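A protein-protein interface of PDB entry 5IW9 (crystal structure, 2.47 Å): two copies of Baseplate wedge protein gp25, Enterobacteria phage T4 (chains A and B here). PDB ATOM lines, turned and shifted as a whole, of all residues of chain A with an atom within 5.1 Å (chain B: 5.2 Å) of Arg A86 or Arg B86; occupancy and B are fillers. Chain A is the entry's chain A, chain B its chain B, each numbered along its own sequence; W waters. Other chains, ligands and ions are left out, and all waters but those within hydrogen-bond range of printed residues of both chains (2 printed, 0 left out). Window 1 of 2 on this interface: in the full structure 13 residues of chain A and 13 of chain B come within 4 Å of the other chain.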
ATOM      1  N   GLY A  27     -11.548 -23.326 -11.533  1.00  0.00           N
ATOM      2  CA  GLY A  27     -10.119 -23.261 -11.799  1.00  0.00           C
ATOM      3  C   GLY A  27      -9.747 -23.904 -13.122  1.00  0.00           C
ATOM      4  O   GLY A  27      -9.017 -23.320 -13.929  1.00  0.00           O
ATOM      5  N   SER A  30     -10.963 -21.761 -16.099  1.00  0.00           N
ATOM      6  CA  SER A  30     -10.142 -20.577 -16.318  1.00  0.00           C
ATOM      7  C   SER A  30      -8.775 -20.947 -16.877  1.00  0.00           C
ATOM      8  O   SER A  30      -8.188 -20.167 -17.638  1.00  0.00           O
ATOM      9  CB  SER A  30      -9.990 -19.784 -15.018  1.00  0.00           C
ATOM     10  OG  SER A  30      -9.183 -20.477 -14.082  1.00  0.00           O
ATOM     11  N   ILE A  31      -8.260 -22.128 -16.522  1.00  0.00           N
ATOM     12  CA  ILE A  31      -6.982 -22.567 -17.072  1.00  0.00           C
ATOM     13  C   ILE A  31      -7.120 -22.905 -18.552  1.00  0.00           C
ATOM     14  O   ILE A  31      -6.256 -22.552 -19.361  1.00  0.00           O
ATOM     15  CB  ILE A  31      -6.429 -23.755 -16.262  1.00  0.00           C
ATOM     16  CG1 ILE A  31      -5.893 -23.268 -14.913  1.00  0.00           C
ATOM     17  CG2 ILE A  31      -5.338 -24.481 -17.044  1.00  0.00           C
ATOM     18  CD1 ILE A  31      -5.725 -24.373 -13.894  1.00  0.00           C
ATOM     19  N   SER A  34      -7.425 -19.717 -20.410  1.00  0.00           N
ATOM     20  CA  SER A  34      -6.105 -19.093 -20.436  1.00  0.00           C
ATOM     21  C   SER A  34      -5.218 -19.725 -21.503  1.00  0.00           C
ATOM     22  O   SER A  34      -4.534 -19.017 -22.255  1.00  0.00           O
ATOM     23  CB  SER A  34      -5.452 -19.196 -19.057  1.00  0.00           C
ATOM     24  OG  SER A  34      -4.086 -18.810 -19.103  1.00  0.00           O
ATOM     25  N   GLU A  84       1.230 -19.579 -17.985  1.00  0.00           N
ATOM     26  CA  GLU A  84       0.208 -20.310 -17.235  1.00  0.00           C
ATOM     27  C   GLU A  84       0.893 -21.161 -16.178  1.00  0.00           C
ATOM     28  O   GLU A  84       1.089 -22.368 -16.355  1.00  0.00           O
ATOM     29  CB  GLU A  84      -0.659 -21.164 -18.164  1.00  0.00           C
ATOM     30  CG  GLU A  84      -1.874 -21.766 -17.477  1.00  0.00           C
ATOM     31  CD  GLU A  84      -2.494 -20.824 -16.458  1.00  0.00           C
ATOM     32  OE1 GLU A  84      -2.186 -20.955 -15.256  1.00  0.00           O
ATOM     33  OE2 GLU A  84      -3.281 -19.944 -16.857  1.00  0.00           O
ATOM     34  N   PRO A  85       1.274 -20.556 -15.050  1.00  0.00           N
ATOM     35  CA  PRO A  85       2.026 -21.302 -14.027  1.00  0.00           C
ATOM     36  C   PRO A  85       1.183 -22.286 -13.230  1.00  0.00           C
ATOM     37  O   PRO A  85       1.749 -23.041 -12.431  1.00  0.00           O
ATOM     38  CB  PRO A  85       2.582 -20.194 -13.125  1.00  0.00           C
ATOM     39  CG  PRO A  85       1.580 -19.091 -13.253  1.00  0.00           C
ATOM     40  CD  PRO A  85       1.071 -19.146 -14.670  1.00  0.00           C
ATOM     41  N   ARG A  86      -0.138 -22.304 -13.410  1.00  0.00           N
ATOM     42  CA  ARG A  86      -0.984 -23.259 -12.705  1.00  0.00           C
ATOM     43  C   ARG A  86      -0.942 -24.654 -13.316  1.00  0.00           C
ATOM     44  O   ARG A  86      -1.502 -25.588 -12.732  1.00  0.00           O
ATOM     45  CB  ARG A  86      -2.431 -22.751 -12.669  1.00  0.00           C
ATOM     46  CG  ARG A  86      -2.640 -21.543 -11.767  1.00  0.00           C
ATOM     47  CD  ARG A  86      -4.021 -20.922 -11.970  1.00  0.00           C
ATOM     48  NE  ARG A  86      -4.183 -20.393 -13.320  1.00  0.00           N
ATOM     49  CZ  ARG A  86      -5.319 -19.896 -13.802  1.00  0.00           C
ATOM     50  NH1 ARG A  86      -6.406 -19.858 -13.042  1.00  0.00           N
ATOM     51  NH2 ARG A  86      -5.367 -19.437 -15.045  1.00  0.00           N
ATOM     52  N   ILE A  87      -0.292 -24.819 -14.463  1.00  0.00           N
ATOM     53  CA  ILE A  87      -0.183 -26.116 -15.123  1.00  0.00           C
ATOM     54  C   ILE A  87       1.068 -26.826 -14.623  1.00  0.00           C
ATOM     55  O   ILE A  87       2.173 -26.274 -14.676  1.00  0.00           O
ATOM     56  CB  ILE A  87      -0.156 -25.951 -16.649  1.00  0.00           C
ATOM     57  CG1 ILE A  87      -1.577 -25.746 -17.178  1.00  0.00           C
ATOM     58  CG2 ILE A  87       0.515 -27.150 -17.317  1.00  0.00           C
ATOM     59  CD1 ILE A  87      -1.635 -25.458 -18.650  1.00  0.00           C
ATOM     60  N   ASP A  88       0.892 -28.053 -14.134  1.00  0.00           N
ATOM     61  CA  ASP A  88       2.002 -28.855 -13.635  1.00  0.00           C
ATOM     62  C   ASP A  88       2.630 -29.663 -14.763  1.00  0.00           C
ATOM     63  O   ASP A  88       3.564 -29.198 -15.423  1.00  0.00           O
ATOM     64  CB  ASP A  88       1.528 -29.783 -12.515  1.00  0.00           C
ATOM     65  CG  ASP A  88       2.648 -30.622 -11.940  1.00  0.00           C
ATOM     66  OD1 ASP A  88       3.790 -30.123 -11.873  1.00  0.00           O
ATOM     67  OD2 ASP A  88       2.385 -31.780 -11.557  1.00  0.00           O
ATOM     68  N   SER A 110      -1.727 -31.167 -16.329  1.00  0.00           N
ATOM     69  CA  SER A 110      -2.306 -31.320 -15.003  1.00  0.00           C
ATOM     70  C   SER A 110      -2.210 -29.994 -14.263  1.00  0.00           C
ATOM     71  O   SER A 110      -1.323 -29.178 -14.531  1.00  0.00           O
ATOM     72  CB  SER A 110      -1.609 -32.429 -14.202  1.00  0.00           C
ATOM     73  OG  SER A 110      -0.251 -32.112 -13.964  1.00  0.00           O
ATOM     74  N   VAL A 111      -3.139 -29.787 -13.328  1.00  0.00           N
ATOM     75  CA  VAL A 111      -3.213 -28.562 -12.541  1.00  0.00           C
ATOM     76  C   VAL A 111      -2.405 -28.740 -11.263  1.00  0.00           C
ATOM     77  O   VAL A 111      -2.382 -29.829 -10.676  1.00  0.00           O
ATOM     78  CB  VAL A 111      -4.680 -28.200 -12.237  1.00  0.00           C
ATOM     79  CG1 VAL A 111      -4.769 -26.905 -11.432  1.00  0.00           C
ATOM     80  CG2 VAL A 111      -5.471 -28.085 -13.530  1.00  0.00           C
ATOM     81  N   ILE A 112      -1.739 -27.663 -10.831  1.00  0.00           N
ATOM     82  CA  ILE A 112      -0.888 -27.713  -9.641  1.00  0.00           C
ATOM     83  C   ILE A 112      -1.640 -28.295  -8.449  1.00  0.00           C
ATOM     84  O   ILE A 112      -1.089 -29.092  -7.679  1.00  0.00           O
ATOM     85  CB  ILE A 112      -0.334 -26.311  -9.322  1.00  0.00           C
ATOM     86  CG1 ILE A 112       0.653 -25.864 -10.400  1.00  0.00           C
ATOM     87  CG2 ILE A 112       0.337 -26.300  -7.955  1.00  0.00           C
ATOM     88  CD1 ILE A 112       1.854 -26.766 -10.536  1.00  0.00           C
ATOM     89  N   GLY B  27       3.872 -14.580 -12.032  1.00  0.00           N
ATOM     90  CA  GLY B  27       2.452 -14.819 -11.840  1.00  0.00           C
ATOM     91  C   GLY B  27       1.618 -13.577 -12.087  1.00  0.00           C
ATOM     92  O   GLY B  27       0.533 -13.653 -12.665  1.00  0.00           O
ATOM     93  N   SER B  30       1.365 -13.016 -15.820  1.00  0.00           N
ATOM     94  CA  SER B  30       0.391 -13.929 -16.409  1.00  0.00           C
ATOM     95  C   SER B  30      -1.037 -13.540 -16.040  1.00  0.00           C
ATOM     96  O   SER B  30      -1.954 -13.711 -16.855  1.00  0.00           O
ATOM     97  CB  SER B  30       0.692 -15.371 -15.991  1.00  0.00           C
ATOM     98  OG  SER B  30       0.378 -15.597 -14.630  1.00  0.00           O
ATOM     99  N   ILE B  31      -1.241 -12.988 -14.840  1.00  0.00           N
ATOM    100  CA  ILE B  31      -2.570 -12.537 -14.438  1.00  0.00           C
ATOM    101  C   ILE B  31      -3.017 -11.353 -15.284  1.00  0.00           C
ATOM    102  O   ILE B  31      -4.165 -11.303 -15.739  1.00  0.00           O
ATOM    103  CB  ILE B  31      -2.596 -12.194 -12.936  1.00  0.00           C
ATOM    104  CG1 ILE B  31      -2.563 -13.468 -12.092  1.00  0.00           C
ATOM    105  CG2 ILE B  31      -3.829 -11.349 -12.596  1.00  0.00           C
ATOM    106  CD1 ILE B  31      -2.264 -13.214 -10.630  1.00  0.00           C
ATOM    107  N   SER B  34      -3.975 -12.615 -18.668  1.00  0.00           N
ATOM    108  CA  SER B  34      -5.279 -13.272 -18.590  1.00  0.00           C
ATOM    109  C   SER B  34      -6.410 -12.249 -18.515  1.00  0.00           C
ATOM    110  O   SER B  34      -7.447 -12.405 -19.174  1.00  0.00           O
ATOM    111  CB  SER B  34      -5.312 -14.212 -17.383  1.00  0.00           C
ATOM    112  OG  SER B  34      -6.638 -14.476 -16.963  1.00  0.00           O
ATOM    113  N   GLU B  84     -10.930 -15.429 -13.582  1.00  0.00           N
ATOM    114  CA  GLU B  84      -9.592 -15.189 -13.042  1.00  0.00           C
ATOM    115  C   GLU B  84      -9.654 -15.330 -11.531  1.00  0.00           C
ATOM    116  O   GLU B  84      -9.698 -14.338 -10.794  1.00  0.00           O
ATOM    117  CB  GLU B  84      -9.055 -13.818 -13.459  1.00  0.00           C
ATOM    118  CG  GLU B  84      -7.605 -13.600 -13.046  1.00  0.00           C
ATOM    119  CD  GLU B  84      -6.755 -14.845 -13.248  1.00  0.00           C
ATOM    120  OE1 GLU B  84      -6.357 -15.118 -14.399  1.00  0.00           O
ATOM    121  OE2 GLU B  84      -6.502 -15.562 -12.256  1.00  0.00           O
ATOM    122  N   PRO B  85      -9.654 -16.569 -11.027  1.00  0.00           N
ATOM    123  CA  PRO B  85      -9.795 -16.777  -9.577  1.00  0.00           C
ATOM    124  C   PRO B  85      -8.565 -16.400  -8.768  1.00  0.00           C
ATOM    125  O   PRO B  85      -8.624 -16.466  -7.534  1.00  0.00           O
ATOM    126  CB  PRO B  85     -10.086 -18.280  -9.470  1.00  0.00           C
ATOM    127  CG  PRO B  85      -9.423 -18.865 -10.680  1.00  0.00           C
ATOM    128  CD  PRO B  85      -9.583 -17.839 -11.769  1.00  0.00           C
ATOM    129  N   ARG B  86      -7.459 -16.015  -9.401  1.00  0.00           N
ATOM    130  CA  ARG B  86      -6.291 -15.576  -8.648  1.00  0.00           C
ATOM    131  C   ARG B  86      -6.411 -14.136  -8.165  1.00  0.00           C
ATOM    132  O   ARG B  86      -5.575 -13.695  -7.368  1.00  0.00           O
ATOM    133  CB  ARG B  86      -5.021 -15.733  -9.492  1.00  0.00           C
ATOM    134  CG  ARG B  86      -4.631 -17.180  -9.762  1.00  0.00           C
ATOM    135  CD  ARG B  86      -3.541 -17.286 -10.818  1.00  0.00           C
ATOM    136  NE  ARG B  86      -4.025 -16.890 -12.135  1.00  0.00           N
ATOM    137  CZ  ARG B  86      -3.266 -16.814 -13.222  1.00  0.00           C
ATOM    138  NH1 ARG B  86      -1.970 -17.102 -13.155  1.00  0.00           N
ATOM    139  NH2 ARG B  86      -3.801 -16.441 -14.379  1.00  0.00           N
ATOM    140  N   ILE B  87      -7.427 -13.407  -8.612  1.00  0.00           N
ATOM    141  CA  ILE B  87      -7.618 -12.013  -8.227  1.00  0.00           C
ATOM    142  C   ILE B  87      -8.481 -11.965  -6.972  1.00  0.00           C
ATOM    143  O   ILE B  87      -9.593 -12.506  -6.948  1.00  0.00           O
ATOM    144  CB  ILE B  87      -8.244 -11.203  -9.372  1.00  0.00           C
ATOM    145  CG1 ILE B  87      -7.188 -10.935 -10.450  1.00  0.00           C
ATOM    146  CG2 ILE B  87      -8.852  -9.906  -8.853  1.00  0.00           C
ATOM    147  CD1 ILE B  87      -7.660 -10.059 -11.577  1.00  0.00           C
ATOM    148  N   ASP B  88      -7.959 -11.332  -5.923  1.00  0.00           N
ATOM    149  CA  ASP B  88      -8.677 -11.191  -4.662  1.00  0.00           C
ATOM    150  C   ASP B  88      -9.532  -9.929  -4.677  1.00  0.00           C
ATOM    151  O   ASP B  88     -10.687  -9.963  -5.112  1.00  0.00           O
ATOM    152  CB  ASP B  88      -7.690 -11.168  -3.491  1.00  0.00           C
ATOM    153  CG  ASP B  88      -8.378 -11.043  -2.147  1.00  0.00           C
ATOM    154  OD1 ASP B  88      -9.509 -11.553  -2.004  1.00  0.00           O
ATOM    155  OD2 ASP B  88      -7.786 -10.430  -1.236  1.00  0.00           O
ATOM    156  N   SER B 110      -5.930  -7.084  -6.288  1.00  0.00           N
ATOM    157  CA  SER B 110      -4.852  -7.738  -5.567  1.00  0.00           C
ATOM    158  C   SER B 110      -4.821  -9.208  -5.957  1.00  0.00           C
ATOM    159  O   SER B 110      -5.803  -9.757  -6.463  1.00  0.00           O
ATOM    160  CB  SER B 110      -5.013  -7.581  -4.047  1.00  0.00           C
ATOM    161  OG  SER B 110      -6.211  -8.185  -3.593  1.00  0.00           O
ATOM    162  N   VAL B 111      -3.674  -9.838  -5.730  1.00  0.00           N
ATOM    163  CA  VAL B 111      -3.480 -11.250  -6.038  1.00  0.00           C
ATOM    164  C   VAL B 111      -3.671 -12.057  -4.762  1.00  0.00           C
ATOM    165  O   VAL B 111      -3.336 -11.606  -3.659  1.00  0.00           O
ATOM    166  CB  VAL B 111      -2.092 -11.495  -6.667  1.00  0.00           C
ATOM    167  CG1 VAL B 111      -1.907 -12.961  -7.031  1.00  0.00           C
ATOM    168  CG2 VAL B 111      -1.912 -10.617  -7.894  1.00  0.00           C
ATOM    169  N   ILE B 112      -4.222 -13.265  -4.920  1.00  0.00           N
ATOM    170  CA  ILE B 112      -4.556 -14.125  -3.784  1.00  0.00           C
ATOM    171  C   ILE B 112      -3.338 -14.384  -2.903  1.00  0.00           C
ATOM    172  O   ILE B 112      -3.438 -14.373  -1.669  1.00  0.00           O
ATOM    173  CB  ILE B 112      -5.176 -15.443  -4.290  1.00  0.00           C
ATOM    174  CG1 ILE B 112      -6.625 -15.222  -4.733  1.00  0.00           C
ATOM    175  CG2 ILE B 112      -5.107 -16.528  -3.222  1.00  0.00           C
ATOM    176  CD1 ILE B 112      -7.555 -14.854  -3.604  1.00  0.00           C
HETATM  177  O   HOH W   1      -2.228 -17.482 -16.410  1.00  0.00           O
HETATM  178  O   HOH W   2      -7.444 -17.447 -15.090  1.00  0.00           O
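The guanidinium group (NH2) of Arg B86 sits close to the guanidinium group (NH2) of Arg A86, 3.4 Å away.
The side-chain hydroxyl (OG) of Ser A30 sits at hydrogen-bond distance from the guanidinium group (NH1) of Arg A86 (3.0 Å). The side-chain carboxylate (OE2) of Glu B84 lies within salt-bridge range of the guanidinium group (NE) of Arg B86 (2.8 Å). OE2 of Glu A84 is in salt-bridge range of NH2 of Arg A86, at 2.8 Å. The backbone NH (N) of Ile A112 sits at hydrogen-bond distance from the backbone carbonyl oxygen (O) of Arg A86. The guanidinium group (NH1) of Arg B86 lies within hydrogen-bond range of the side-chain hydroxyl (OG) of Ser B30 (3.2 Å). The backbone carbonyl oxygen (O) of Gly A27 lies within hydrogen-bond range of the side-chain hydroxyl (OG) of Ser A30, 2.9 Å away.
Among the printed residues, merely in contact across the chains: Ser A30 with Pro B85 (3.5 Å), Pro A85 with Ser B30 (3.6 Å), Arg A86 with Pro B85 (3.96 Å) and Pro A85 with Arg B86 (3.96 Å).
Of the printed residues of chain B, Ser A30 touches Pro B85 (3.5 Å). Of the printed residues of chain B, Pro A85 touches Ser B30 and Arg B86. Arg A86 touches just these residues of chain B: Pro B85 (3.96 Å) and Arg B86 (3.4 Å). Ile A112 touches none of the printed residues of chain B. Of the printed residues of chain A, Pro B85 touches Ser A30 and Arg A86. Arg B86 touches just these residues of chain A: Pro A85 and Arg A86. Ile B112 touches none of the printed residues of chain A. The nearest residue of chain B that does not touch Arg A86 is Glu B84 (4.4 Å). The nearest residue of chain A that does not touch Arg B86 is Glu A84 (4.3 Å). The nearest printed residue of chain B that does not touch Ser A30 is Glu B84 (4.7 Å).
Of the 12 printed residues of chain A, 3 touch a printed residue of chain B. Printed residues of chain A that touch a printed residue of chain B: Ser A30, Pro A85 and Arg A86. Of the 12 printed residues of chain B, 3 touch a printed residue of chain A. Along chain B the printed residues that touch a printed residue of chain A span positions 30 to 86.
Ser A30 touches Pro B85, and with the chains exchanged Pro A85 touches Ser B30. Pro A85 touches Arg B86, and with the chains exchanged Arg A86 touches Pro B85. Arg A86 touches its own counterpart, Arg B86. 12 positions are printed for both chains. Of the 5 pairs that touch across the chains among the printed residues, 5 have their exchanged pair printed and touching as well.
Water W2 lies within hydrogen-bond range of the side-chain carboxylate (OE1) of Glu B84 (2.7 Å) and the guanidinium group (NH2) of Arg A86 (2.9 Å). Water W1 lies within hydrogen-bond range of the side-chain carboxylate of Glu A84 and the guanidinium group of Arg B86.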
